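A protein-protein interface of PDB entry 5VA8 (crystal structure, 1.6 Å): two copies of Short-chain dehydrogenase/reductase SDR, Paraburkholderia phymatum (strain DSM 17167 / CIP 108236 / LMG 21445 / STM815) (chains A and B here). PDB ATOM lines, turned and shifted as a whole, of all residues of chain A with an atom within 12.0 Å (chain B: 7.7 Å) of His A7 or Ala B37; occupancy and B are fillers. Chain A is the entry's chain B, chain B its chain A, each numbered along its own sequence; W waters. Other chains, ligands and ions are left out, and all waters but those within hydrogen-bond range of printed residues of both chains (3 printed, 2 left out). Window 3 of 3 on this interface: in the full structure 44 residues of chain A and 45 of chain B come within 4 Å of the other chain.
The side-chain carboxylate (OE1) of Glu A38 is in hydrogen-bond range of the backbone NH (N) of His B8 (3.3 Å). The backbone carbonyl oxygen (O) of Met B9 lies within hydrogen-bond range of the backbone NH (N) of Met A9 (2.8 Å). The backbone NH (N) of Met B9 is in hydrogen-bond range of the side-chain carboxylate (OE1) of Glu A38 (3.5 Å). The side-chain carboxylate (OE1) of Glu B38 is in hydrogen-bond range of the backbone NH (N) of His A8.
The side-chain carboxylate (OD1) of Asp B10 is in hydrogen-bond range of the backbone NH (N) of Gly B12 (2.8 Å). The backbone carbonyl oxygen (O) of Asp A10 is in hydrogen-bond range of a ring nitrogen (NE2) of His A247 (2.6 Å).
Asp B10 touches His A7 (OD1 to O, 3.5 Å). His A8 touches His B8 (CB to CB, 3.3 Å). CA of His A8 touches O of Met B9, 3.2 Å away. O of Met A9 touches CA of His B8 (3.2 Å). CE of Met A9 touches CD1 of Leu B11, at 3.8 Å. Met A9 touches Glu B38. CE of Met A9 touches O of Arg B238 (3.7 Å). Arg A238 touches Met B9. Arg B238 touches Phe A242. His A247 touches Arg B238.
His A7 touches just these residues of chain B: Asp B10, Ala B37 and Glu B38. Of the printed residues of chain B, Met A9 touches His B8 (3.2 Å), Met B9 (2.8 Å), Leu B11 (3.8 Å), Glu B38 (3.5 Å) and Arg B238 (3.7 Å). Of the printed residues of chain B, Glu A38 touches His B8 (3.3 Å) and Met B9 (3.5 Å). Of the printed residues of chain B, Arg A238 touches Met B9 (3.7 Å). Of the printed residues of chain B, His A247 touches Arg B238. Asp B10 touches just one residue of chain A: His A7 (3.5 Å). Leu B11 touches just one residue of chain A: Met A9 (3.8 Å). No residue of chain A comes within 4 Å of Ala B14. No residue of chain A comes within 4 Å of Ala B34. Ala B36 touches none of the printed residues of chain A. Printed residues of chain A within 4 Å of Ala B37: His A7 (3.2 Å). Glu B38 touches just these residues of chain A: His A7 (3.7 Å), His A8 (3.2 Å) and Met A9 (3.5 Å). No residue of chain A comes within 4 Å of Ala B63. Printed residues of chain A within 4 Å of Arg B238: Met A9 (3.7 Å), Phe A242 (3.7 Å) and His A247 (3.9 Å). The nearest residue of chain B that does not touch His A7 is Ala B14 (4.3 Å). The nearest printed residue of chain B that does not touch Met A9 is Ala B241 (4.03 Å).
Hydrophobic or aromatic side chains of chain A within 4 Å of the printed part of chain B: His A7, His A8, Met A9, Phe A242 and His A247. Among the printed residues, no Asp or Glu carboxylate lies within 4 Å of a Lys or Arg side-chain nitrogen of the other chain.
His B8 touches its own counterpart, His A8. His A8 touches Met B9, and with the chains exchanged Met A9 touches His B8. Met A9 touches Glu B38, and with the chains exchanged Glu A38 touches Met B9. Met A9 touches Arg B238, and with the chains exchanged Arg A238 touches Met B9. 7 positions are printed for both chains. Of the 16 pairs that touch across the chains among the printed residues, 10 have their exchanged pair printed and touching as well.
Water W1 lies within hydrogen-bond range of OE1 of Glu B38 (2.5 Å), N of Leu B11 (2.8 Å), O of His A7 (2.9 Å) and N of His A8 (3.3 Å). Water W2 lies within hydrogen-bond range of OE2 of Glu B38 and O of His A8. Water W3 lies within hydrogen-bond range of OE2 of Glu A38 (2.9 Å) and O of His B8 (3.1 Å).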
ATOM      1  N   HIS A   7      16.121 -23.629  32.705  1.00  0.00           N
ATOM      2  CA  HIS A   7      17.254 -23.320  31.843  1.00  0.00           C
ATOM      3  C   HIS A   7      16.847 -23.340  30.374  1.00  0.00           C
ATOM      4  O   HIS A   7      15.776 -22.848  30.012  1.00  0.00           O
ATOM      5  CB  HIS A   7      18.397 -24.305  32.088  1.00  0.00           C
ATOM      6  N   HIS A   8      17.701 -23.918  29.532  1.00  0.00           N
ATOM      7  CA  HIS A   8      17.438 -23.950  28.101  1.00  0.00           C
ATOM      8  C   HIS A   8      18.445 -24.873  27.424  1.00  0.00           C
ATOM      9  O   HIS A   8      19.625 -24.883  27.787  1.00  0.00           O
ATOM     10  CB  HIS A   8      17.503 -22.538  27.507  1.00  0.00           C
ATOM     11  N   MET A   9      17.969 -25.641  26.442  1.00  0.00           N
ATOM     12  CA  MET A   9      18.767 -26.659  25.765  1.00  0.00           C
ATOM     13  C   MET A   9      19.345 -26.082  24.479  1.00  0.00           C
ATOM     14  O   MET A   9      18.597 -25.610  23.615  1.00  0.00           O
ATOM     15  CB  MET A   9      17.921 -27.898  25.458  1.00  0.00           C
ATOM     16  CG  MET A   9      18.708 -29.078  24.890  1.00  0.00           C
ATOM     17  SD  MET A   9      17.657 -30.361  24.160  1.00  0.00           S
ATOM     18  CE  MET A   9      16.960 -31.092  25.642  1.00  0.00           C
ATOM     19  N   ASP A  10      20.670 -26.146  24.343  1.00  0.00           N
ATOM     20  CA  ASP A  10      21.363 -25.623  23.165  1.00  0.00           C
ATOM     21  C   ASP A  10      21.318 -26.674  22.063  1.00  0.00           C
ATOM     22  O   ASP A  10      21.959 -27.722  22.168  1.00  0.00           O
ATOM     23  CB  ASP A  10      22.799 -25.251  23.530  1.00  0.00           C
ATOM     24  CG  ASP A  10      23.576 -24.638  22.369  1.00  0.00           C
ATOM     25  OD1 ASP A  10      23.027 -24.496  21.258  1.00  0.00           O
ATOM     26  OD2 ASP A  10      24.760 -24.293  22.582  1.00  0.00           O
ATOM     27  N   LEU A  11      20.572 -26.394  20.998  1.00  0.00           N
ATOM     28  CA  LEU A  11      20.432 -27.359  19.914  1.00  0.00           C
ATOM     29  C   LEU A  11      21.624 -27.372  18.966  1.00  0.00           C
ATOM     30  O   LEU A  11      21.676 -28.230  18.078  1.00  0.00           O
ATOM     31  CB  LEU A  11      19.149 -27.090  19.129  1.00  0.00           C
ATOM     32  CG  LEU A  11      17.860 -27.248  19.939  1.00  0.00           C
ATOM     33  CD1 LEU A  11      16.665 -27.285  18.997  1.00  0.00           C
ATOM     34  CD2 LEU A  11      17.904 -28.481  20.818  1.00  0.00           C
ATOM     35  N   ALA A  37      14.375 -19.433  16.172  1.00  0.00           N
ATOM     36  CA  ALA A  37      14.598 -19.203  17.595  1.00  0.00           C
ATOM     37  C   ALA A  37      15.890 -19.844  18.084  1.00  0.00           C
ATOM     38  O   ALA A  37      16.448 -19.400  19.094  1.00  0.00           O
ATOM     39  CB  ALA A  37      13.414 -19.736  18.402  1.00  0.00           C
ATOM     40  N   GLU A  38      16.377 -20.872  17.393  1.00  0.00           N
ATOM     41  CA  GLU A  38      17.646 -21.502  17.724  1.00  0.00           C
ATOM     42  C   GLU A  38      18.796 -20.958  16.886  1.00  0.00           C
ATOM     43  O   GLU A  38      19.869 -21.565  16.855  1.00  0.00           O
ATOM     44  CB  GLU A  38      17.537 -23.018  17.565  1.00  0.00           C
ATOM     45  CG  GLU A  38      16.358 -23.642  18.323  1.00  0.00           C
ATOM     46  CD  GLU A  38      16.313 -23.277  19.806  1.00  0.00           C
ATOM     47  OE1 GLU A  38      17.380 -23.261  20.457  1.00  0.00           O
ATOM     48  OE2 GLU A  38      15.206 -23.000  20.322  1.00  0.00           O
ATOM     49  N   ARG A 238       8.603 -27.019  17.576  1.00  0.00           N
ATOM     50  CA  ARG A 238       9.634 -27.384  18.550  1.00  0.00           C
ATOM     51  C   ARG A 238      10.109 -28.817  18.347  1.00  0.00           C
ATOM     52  O   ARG A 238      11.306 -29.101  18.477  1.00  0.00           O
ATOM     53  CB  ARG A 238       9.128 -27.217  19.982  1.00  0.00           C
ATOM     54  CG  ARG A 238       8.585 -25.842  20.331  1.00  0.00           C
ATOM     55  CD  ARG A 238       9.602 -24.738  20.182  1.00  0.00           C
ATOM     56  NE  ARG A 238       9.037 -23.476  20.661  1.00  0.00           N
ATOM     57  CZ  ARG A 238       9.633 -22.290  20.570  1.00  0.00           C
ATOM     58  NH1 ARG A 238      10.831 -22.175  20.011  1.00  0.00           N
ATOM     59  NH2 ARG A 238       9.019 -21.212  21.044  1.00  0.00           N
ATOM     60  N   PHE A 242      13.939 -29.973  17.449  1.00  0.00           N
ATOM     61  CA  PHE A 242      14.716 -31.005  18.129  1.00  0.00           C
ATOM     62  C   PHE A 242      15.278 -32.010  17.130  1.00  0.00           C
ATOM     63  O   PHE A 242      16.443 -32.407  17.232  1.00  0.00           O
ATOM     64  CB  PHE A 242      13.883 -31.731  19.190  1.00  0.00           C
ATOM     65  CG  PHE A 242      14.688 -32.747  19.956  1.00  0.00           C
ATOM     66  CD1 PHE A 242      15.469 -32.361  21.032  1.00  0.00           C
ATOM     67  CD2 PHE A 242      14.740 -34.069  19.535  1.00  0.00           C
ATOM     68  CE1 PHE A 242      16.246 -33.289  21.717  1.00  0.00           C
ATOM     69  CE2 PHE A 242      15.516 -34.996  20.204  1.00  0.00           C
ATOM     70  CZ  PHE A 242      16.269 -34.610  21.298  1.00  0.00           C
ATOM     71  N   HIS A 247      21.470 -32.987  18.829  1.00  0.00           N
ATOM     72  CA  HIS A 247      21.105 -33.977  19.834  1.00  0.00           C
ATOM     73  C   HIS A 247      20.222 -35.082  19.282  1.00  0.00           C
ATOM     74  O   HIS A 247      19.843 -35.987  20.034  1.00  0.00           O
ATOM     75  CB  HIS A 247      20.403 -33.299  21.019  1.00  0.00           C
ATOM     76  CG  HIS A 247      21.214 -32.208  21.643  1.00  0.00           C
ATOM     77  ND1 HIS A 247      22.479 -32.419  22.142  1.00  0.00           N
ATOM     78  CD2 HIS A 247      20.950 -30.893  21.823  1.00  0.00           C
ATOM     79  CE1 HIS A 247      22.959 -31.281  22.612  1.00  0.00           C
ATOM     80  NE2 HIS A 247      22.049 -30.340  22.431  1.00  0.00           N
ATOM     81  N   HIS B   8      19.021 -21.327  22.619  1.00  0.00           N
ATOM     82  CA  HIS B   8      18.638 -22.427  23.495  1.00  0.00           C
ATOM     83  C   HIS B   8      17.126 -22.430  23.708  1.00  0.00           C
ATOM     84  O   HIS B   8      16.491 -21.372  23.766  1.00  0.00           O
ATOM     85  CB  HIS B   8      19.376 -22.339  24.835  1.00  0.00           C
ATOM     86  N   MET B   9      16.566 -23.636  23.833  1.00  0.00           N
ATOM     87  CA  MET B   9      15.126 -23.859  23.927  1.00  0.00           C
ATOM     88  C   MET B   9      14.716 -24.099  25.377  1.00  0.00           C
ATOM     89  O   MET B   9      15.249 -25.000  26.033  1.00  0.00           O
ATOM     90  CB  MET B   9      14.714 -25.060  23.068  1.00  0.00           C
ATOM     91  CG  MET B   9      13.238 -25.439  23.163  1.00  0.00           C
ATOM     92  SD  MET B   9      12.853 -27.039  22.407  1.00  0.00           S
ATOM     93  CE  MET B   9      13.076 -26.694  20.664  1.00  0.00           C
ATOM     94  N   ASP B  10      13.754 -23.314  25.864  1.00  0.00           N
ATOM     95  CA  ASP B  10      13.284 -23.438  27.244  1.00  0.00           C
ATOM     96  C   ASP B  10      12.258 -24.566  27.337  1.00  0.00           C
ATOM     97  O   ASP B  10      11.171 -24.468  26.760  1.00  0.00           O
ATOM     98  CB  ASP B  10      12.674 -22.114  27.710  1.00  0.00           C
ATOM     99  CG  ASP B  10      12.368 -22.088  29.206  1.00  0.00           C
ATOM    100  OD1 ASP B  10      12.271 -23.154  29.840  1.00  0.00           O
ATOM    101  OD2 ASP B  10      12.204 -20.975  29.751  1.00  0.00           O
ATOM    102  N   LEU B  11      12.588 -25.623  28.080  1.00  0.00           N
ATOM    103  CA  LEU B  11      11.685 -26.763  28.188  1.00  0.00           C
ATOM    104  C   LEU B  11      10.583 -26.564  29.221  1.00  0.00           C
ATOM    105  O   LEU B  11       9.702 -27.426  29.330  1.00  0.00           O
ATOM    106  CB  LEU B  11      12.470 -28.036  28.517  1.00  0.00           C
ATOM    107  CG  LEU B  11      13.496 -28.441  27.452  1.00  0.00           C
ATOM    108  CD1 LEU B  11      14.006 -29.856  27.739  1.00  0.00           C
ATOM    109  CD2 LEU B  11      12.918 -28.321  26.050  1.00  0.00           C
ATOM    110  N   GLY B  12      10.617 -25.470  29.982  1.00  0.00           N
ATOM    111  CA  GLY B  12       9.527 -25.122  30.873  1.00  0.00           C
ATOM    112  C   GLY B  12       9.343 -26.006  32.087  1.00  0.00           C
ATOM    113  O   GLY B  12       8.259 -25.993  32.676  1.00  0.00           O
ATOM    114  N   ILE B  13      10.365 -26.759  32.501  1.00  0.00           N
ATOM    115  CA  ILE B  13      10.193 -27.730  33.577  1.00  0.00           C
ATOM    116  C   ILE B  13      11.130 -27.458  34.754  1.00  0.00           C
ATOM    117  O   ILE B  13      11.306 -28.316  35.615  1.00  0.00           O
ATOM    118  CB  ILE B  13      10.344 -29.173  33.054  1.00  0.00           C
ATOM    119  CG1 ILE B  13      11.661 -29.368  32.283  1.00  0.00           C
ATOM    120  CG2 ILE B  13       9.143 -29.531  32.179  1.00  0.00           C
ATOM    121  CD1 ILE B  13      11.905 -30.835  31.836  1.00  0.00           C
ATOM    122  N   ALA B  14      11.722 -26.268  34.811  1.00  0.00           N
ATOM    123  CA  ALA B  14      12.548 -25.901  35.951  1.00  0.00           C
ATOM    124  C   ALA B  14      11.720 -25.925  37.230  1.00  0.00           C
ATOM    125  O   ALA B  14      10.607 -25.391  37.278  1.00  0.00           O
ATOM    126  CB  ALA B  14      13.159 -24.515  35.742  1.00  0.00           C
ATOM    127  N   GLY B  15      12.270 -26.550  38.269  1.00  0.00           N
ATOM    128  CA  GLY B  15      11.604 -26.619  39.547  1.00  0.00           C
ATOM    129  C   GLY B  15      10.661 -27.791  39.703  1.00  0.00           C
ATOM    130  O   GLY B  15      10.198 -28.049  40.826  1.00  0.00           O
ATOM    131  N   CYS B  31      19.611 -39.531  31.402  1.00  0.00           N
ATOM    132  CA  CYS B  31      18.321 -38.869  31.586  1.00  0.00           C
ATOM    133  C   CYS B  31      18.345 -37.939  32.792  1.00  0.00           C
ATOM    134  O   CYS B  31      17.844 -36.806  32.723  1.00  0.00           O
ATOM    135  CB  CYS B  31      17.200 -39.898  31.740  1.00  0.00           C
ATOM    136  SG  CYS B  31      16.901 -40.878  30.255  1.00  0.00           S
ATOM    137  N   ALA B  32      18.914 -38.400  33.909  1.00  0.00           N
ATOM    138  CA  ALA B  32      18.978 -37.562  35.100  1.00  0.00           C
ATOM    139  C   ALA B  32      19.771 -36.292  34.842  1.00  0.00           C
ATOM    140  O   ALA B  32      19.358 -35.204  35.257  1.00  0.00           O
ATOM    141  CB  ALA B  32      19.593 -38.344  36.263  1.00  0.00           C
ATOM    142  N   GLU B  33      20.920 -36.408  34.169  1.00  0.00           N
ATOM    143  CA  GLU B  33      21.739 -35.230  33.895  1.00  0.00           C
ATOM    144  C   GLU B  33      21.007 -34.252  32.986  1.00  0.00           C
ATOM    145  O   GLU B  33      21.098 -33.034  33.176  1.00  0.00           O
ATOM    146  CB  GLU B  33      23.074 -35.639  33.266  1.00  0.00           C
ATOM    147  CG  GLU B  33      23.909 -36.526  34.192  1.00  0.00           C
ATOM    148  CD  GLU B  33      25.395 -36.482  33.908  1.00  0.00           C
ATOM    149  OE1 GLU B  33      25.988 -35.390  34.044  1.00  0.00           O
ATOM    150  OE2 GLU B  33      25.975 -37.540  33.560  1.00  0.00           O
ATOM    151  N   ALA B  34      20.292 -34.765  31.983  1.00  0.00           N
ATOM    152  CA  ALA B  34      19.615 -33.875  31.042  1.00  0.00           C
ATOM    153  C   ALA B  34      18.446 -33.162  31.704  1.00  0.00           C
ATOM    154  O   ALA B  34      18.232 -31.967  31.464  1.00  0.00           O
ATOM    155  CB  ALA B  34      19.147 -34.661  29.818  1.00  0.00           C
ATOM    156  N   LEU B  35      17.693 -33.866  32.556  1.00  0.00           N
ATOM    157  CA  LEU B  35      16.606 -33.216  33.290  1.00  0.00           C
ATOM    158  C   LEU B  35      17.153 -32.180  34.266  1.00  0.00           C
ATOM    159  O   LEU B  35      16.653 -31.050  34.332  1.00  0.00           O
ATOM    160  CB  LEU B  35      15.753 -34.263  34.017  1.00  0.00           C
ATOM    161  CG  LEU B  35      14.957 -35.196  33.101  1.00  0.00           C
ATOM    162  CD1 LEU B  35      14.388 -36.382  33.886  1.00  0.00           C
ATOM    163  CD2 LEU B  35      13.836 -34.431  32.391  1.00  0.00           C
ATOM    164  N   ALA B  36      18.199 -32.536  35.017  1.00  0.00           N
ATOM    165  CA  ALA B  36      18.802 -31.574  35.940  1.00  0.00           C
ATOM    166  C   ALA B  36      19.305 -30.336  35.205  1.00  0.00           C
ATOM    167  O   ALA B  36      19.202 -29.215  35.723  1.00  0.00           O
ATOM    168  CB  ALA B  36      19.942 -32.236  36.716  1.00  0.00           C
ATOM    169  N   ALA B  37      19.860 -30.518  33.997  1.00  0.00           N
ATOM    170  CA  ALA B  37      20.353 -29.390  33.215  1.00  0.00           C
ATOM    171  C   ALA B  37      19.245 -28.414  32.852  1.00  0.00           C
ATOM    172  O   ALA B  37      19.522 -27.236  32.600  1.00  0.00           O
ATOM    173  CB  ALA B  37      21.034 -29.888  31.936  1.00  0.00           C
ATOM    174  N   GLU B  38      18.001 -28.879  32.808  1.00  0.00           N
ATOM    175  CA  GLU B  38      16.860 -28.010  32.564  1.00  0.00           C
ATOM    176  C   GLU B  38      16.183 -27.579  33.861  1.00  0.00           C
ATOM    177  O   GLU B  38      15.053 -27.079  33.830  1.00  0.00           O
ATOM    178  CB  GLU B  38      15.866 -28.704  31.631  1.00  0.00           C
ATOM    179  CG  GLU B  38      16.486 -29.240  30.330  1.00  0.00           C
ATOM    180  CD  GLU B  38      17.265 -28.192  29.535  1.00  0.00           C
ATOM    181  OE1 GLU B  38      16.934 -26.987  29.602  1.00  0.00           O
ATOM    182  OE2 GLU B  38      18.232 -28.580  28.842  1.00  0.00           O
ATOM    183  N   GLY B  39      16.860 -27.749  34.997  1.00  0.00           N
ATOM    184  CA  GLY B  39      16.375 -27.246  36.262  1.00  0.00           C
ATOM    185  C   GLY B  39      15.460 -28.168  37.027  1.00  0.00           C
ATOM    186  O   GLY B  39      14.867 -27.729  38.019  1.00  0.00           O
ATOM    187  N   VAL B  40      15.331 -29.422  36.611  1.00  0.00           N
ATOM    188  CA  VAL B  40      14.475 -30.385  37.302  1.00  0.00           C
ATOM    189  C   VAL B  40      15.195 -30.910  38.537  1.00  0.00           C
ATOM    190  O   VAL B  40      16.370 -31.287  38.470  1.00  0.00           O
ATOM    191  CB  VAL B  40      14.098 -31.545  36.366  1.00  0.00           C
ATOM    192  CG1 VAL B  40      13.229 -32.564  37.104  1.00  0.00           C
ATOM    193  CG2 VAL B  40      13.386 -31.016  35.117  1.00  0.00           C
ATOM    194  N   VAL B  42      16.013 -33.857  40.760  1.00  0.00           N
ATOM    195  CA  VAL B  42      16.016 -35.268  40.388  1.00  0.00           C
ATOM    196  C   VAL B  42      16.293 -36.131  41.610  1.00  0.00           C
ATOM    197  O   VAL B  42      17.165 -35.824  42.428  1.00  0.00           O
ATOM    198  CB  VAL B  42      17.028 -35.579  39.261  1.00  0.00           C
ATOM    199  CG1 VAL B  42      16.580 -34.915  37.953  1.00  0.00           C
ATOM    200  CG2 VAL B  42      18.437 -35.151  39.656  1.00  0.00           C
ATOM    201  N   ILE B  59      25.941 -34.438  39.700  1.00  0.00           N
ATOM    202  CA  ILE B  59      24.789 -33.708  39.174  1.00  0.00           C
ATOM    203  C   ILE B  59      24.530 -32.451  40.001  1.00  0.00           C
ATOM    204  O   ILE B  59      24.210 -31.387  39.453  1.00  0.00           O
ATOM    205  CB  ILE B  59      23.558 -34.632  39.123  1.00  0.00           C
ATOM    206  CG1 ILE B  59      23.799 -35.765  38.125  1.00  0.00           C
ATOM    207  CG2 ILE B  59      22.300 -33.851  38.733  1.00  0.00           C
ATOM    208  CD1 ILE B  59      22.685 -36.824  38.113  1.00  0.00           C
ATOM    209  N   ASN B  62      27.077 -29.986  38.819  1.00  0.00           N
ATOM    210  CA  ASN B  62      26.872 -29.559  37.439  1.00  0.00           C
ATOM    211  C   ASN B  62      25.643 -28.672  37.294  1.00  0.00           C
ATOM    212  O   ASN B  62      25.665 -27.683  36.547  1.00  0.00           O
ATOM    213  CB  ASN B  62      26.724 -30.775  36.525  1.00  0.00           C
ATOM    214  CG  ASN B  62      28.027 -31.511  36.305  1.00  0.00           C
ATOM    215  OD1 ASN B  62      29.104 -30.994  36.589  1.00  0.00           O
ATOM    216  ND2 ASN B  62      27.930 -32.734  35.791  1.00  0.00           N
ATOM    217  N   ALA B  63      24.554 -29.017  37.977  1.00  0.00           N
ATOM    218  CA  ALA B  63      23.254 -28.454  37.650  1.00  0.00           C
ATOM    219  C   ALA B  63      22.682 -27.523  38.706  1.00  0.00           C
ATOM    220  O   ALA B  63      21.799 -26.721  38.381  1.00  0.00           O
ATOM    221  CB  ALA B  63      22.245 -29.582  37.385  1.00  0.00           C
ATOM    222  N   GLY B  64      23.145 -27.606  39.951  1.00  0.00           N
ATOM    223  CA  GLY B  64      22.635 -26.715  40.973  1.00  0.00           C
ATOM    224  C   GLY B  64      21.192 -26.948  41.355  1.00  0.00           C
ATOM    225  O   GLY B  64      20.549 -26.041  41.886  1.00  0.00           O
ATOM    226  N   VAL B  65      20.659 -28.132  41.082  1.00  0.00           N
ATOM    227  CA  VAL B  65      19.312 -28.487  41.472  1.00  0.00           C
ATOM    228  C   VAL B  65      19.390 -29.356  42.721  1.00  0.00           C
ATOM    229  O   VAL B  65      20.465 -29.774  43.149  1.00  0.00           O
ATOM    230  CB  VAL B  65      18.556 -29.228  40.338  1.00  0.00           C
ATOM    231  CG1 VAL B  65      18.562 -28.403  39.056  1.00  0.00           C
ATOM    232  CG2 VAL B  65      19.190 -30.585  40.096  1.00  0.00           C
ATOM    233  N   ARG B 238      18.865 -36.254  26.304  1.00  0.00           N
ATOM    234  CA  ARG B 238      18.262 -35.067  25.707  1.00  0.00           C
ATOM    235  C   ARG B 238      16.904 -35.387  25.093  1.00  0.00           C
ATOM    236  O   ARG B 238      15.967 -34.589  25.203  1.00  0.00           O
ATOM    237  CB  ARG B 238      19.191 -34.463  24.651  1.00  0.00           C
ATOM    238  CG  ARG B 238      20.580 -34.109  25.148  1.00  0.00           C
ATOM    239  CD  ARG B 238      20.584 -33.024  26.211  1.00  0.00           C
ATOM    240  NE  ARG B 238      21.958 -32.600  26.493  1.00  0.00           N
ATOM    241  CZ  ARG B 238      22.315 -31.788  27.484  1.00  0.00           C
ATOM    242  NH1 ARG B 238      21.404 -31.301  28.316  1.00  0.00           N
ATOM    243  NH2 ARG B 238      23.592 -31.468  27.647  1.00  0.00           N
ATOM    244  N   ALA B 241      14.523 -35.589  27.912  1.00  0.00           N
ATOM    245  CA  ALA B 241      14.160 -34.265  28.410  1.00  0.00           C
ATOM    246  C   ALA B 241      13.143 -33.598  27.496  1.00  0.00           C
ATOM    247  O   ALA B 241      12.205 -32.950  27.973  1.00  0.00           O
ATOM    248  CB  ALA B 241      15.407 -33.390  28.567  1.00  0.00           C
HETATM  249  O   HOH W   1      14.858 -25.592  29.712  1.00  0.00           O
HETATM  250  O   HOH W   2      20.839 -27.444  28.549  1.00  0.00           O
HETATM  251  O   HOH W   3      13.930 -20.975  21.977  1.00  0.00           O
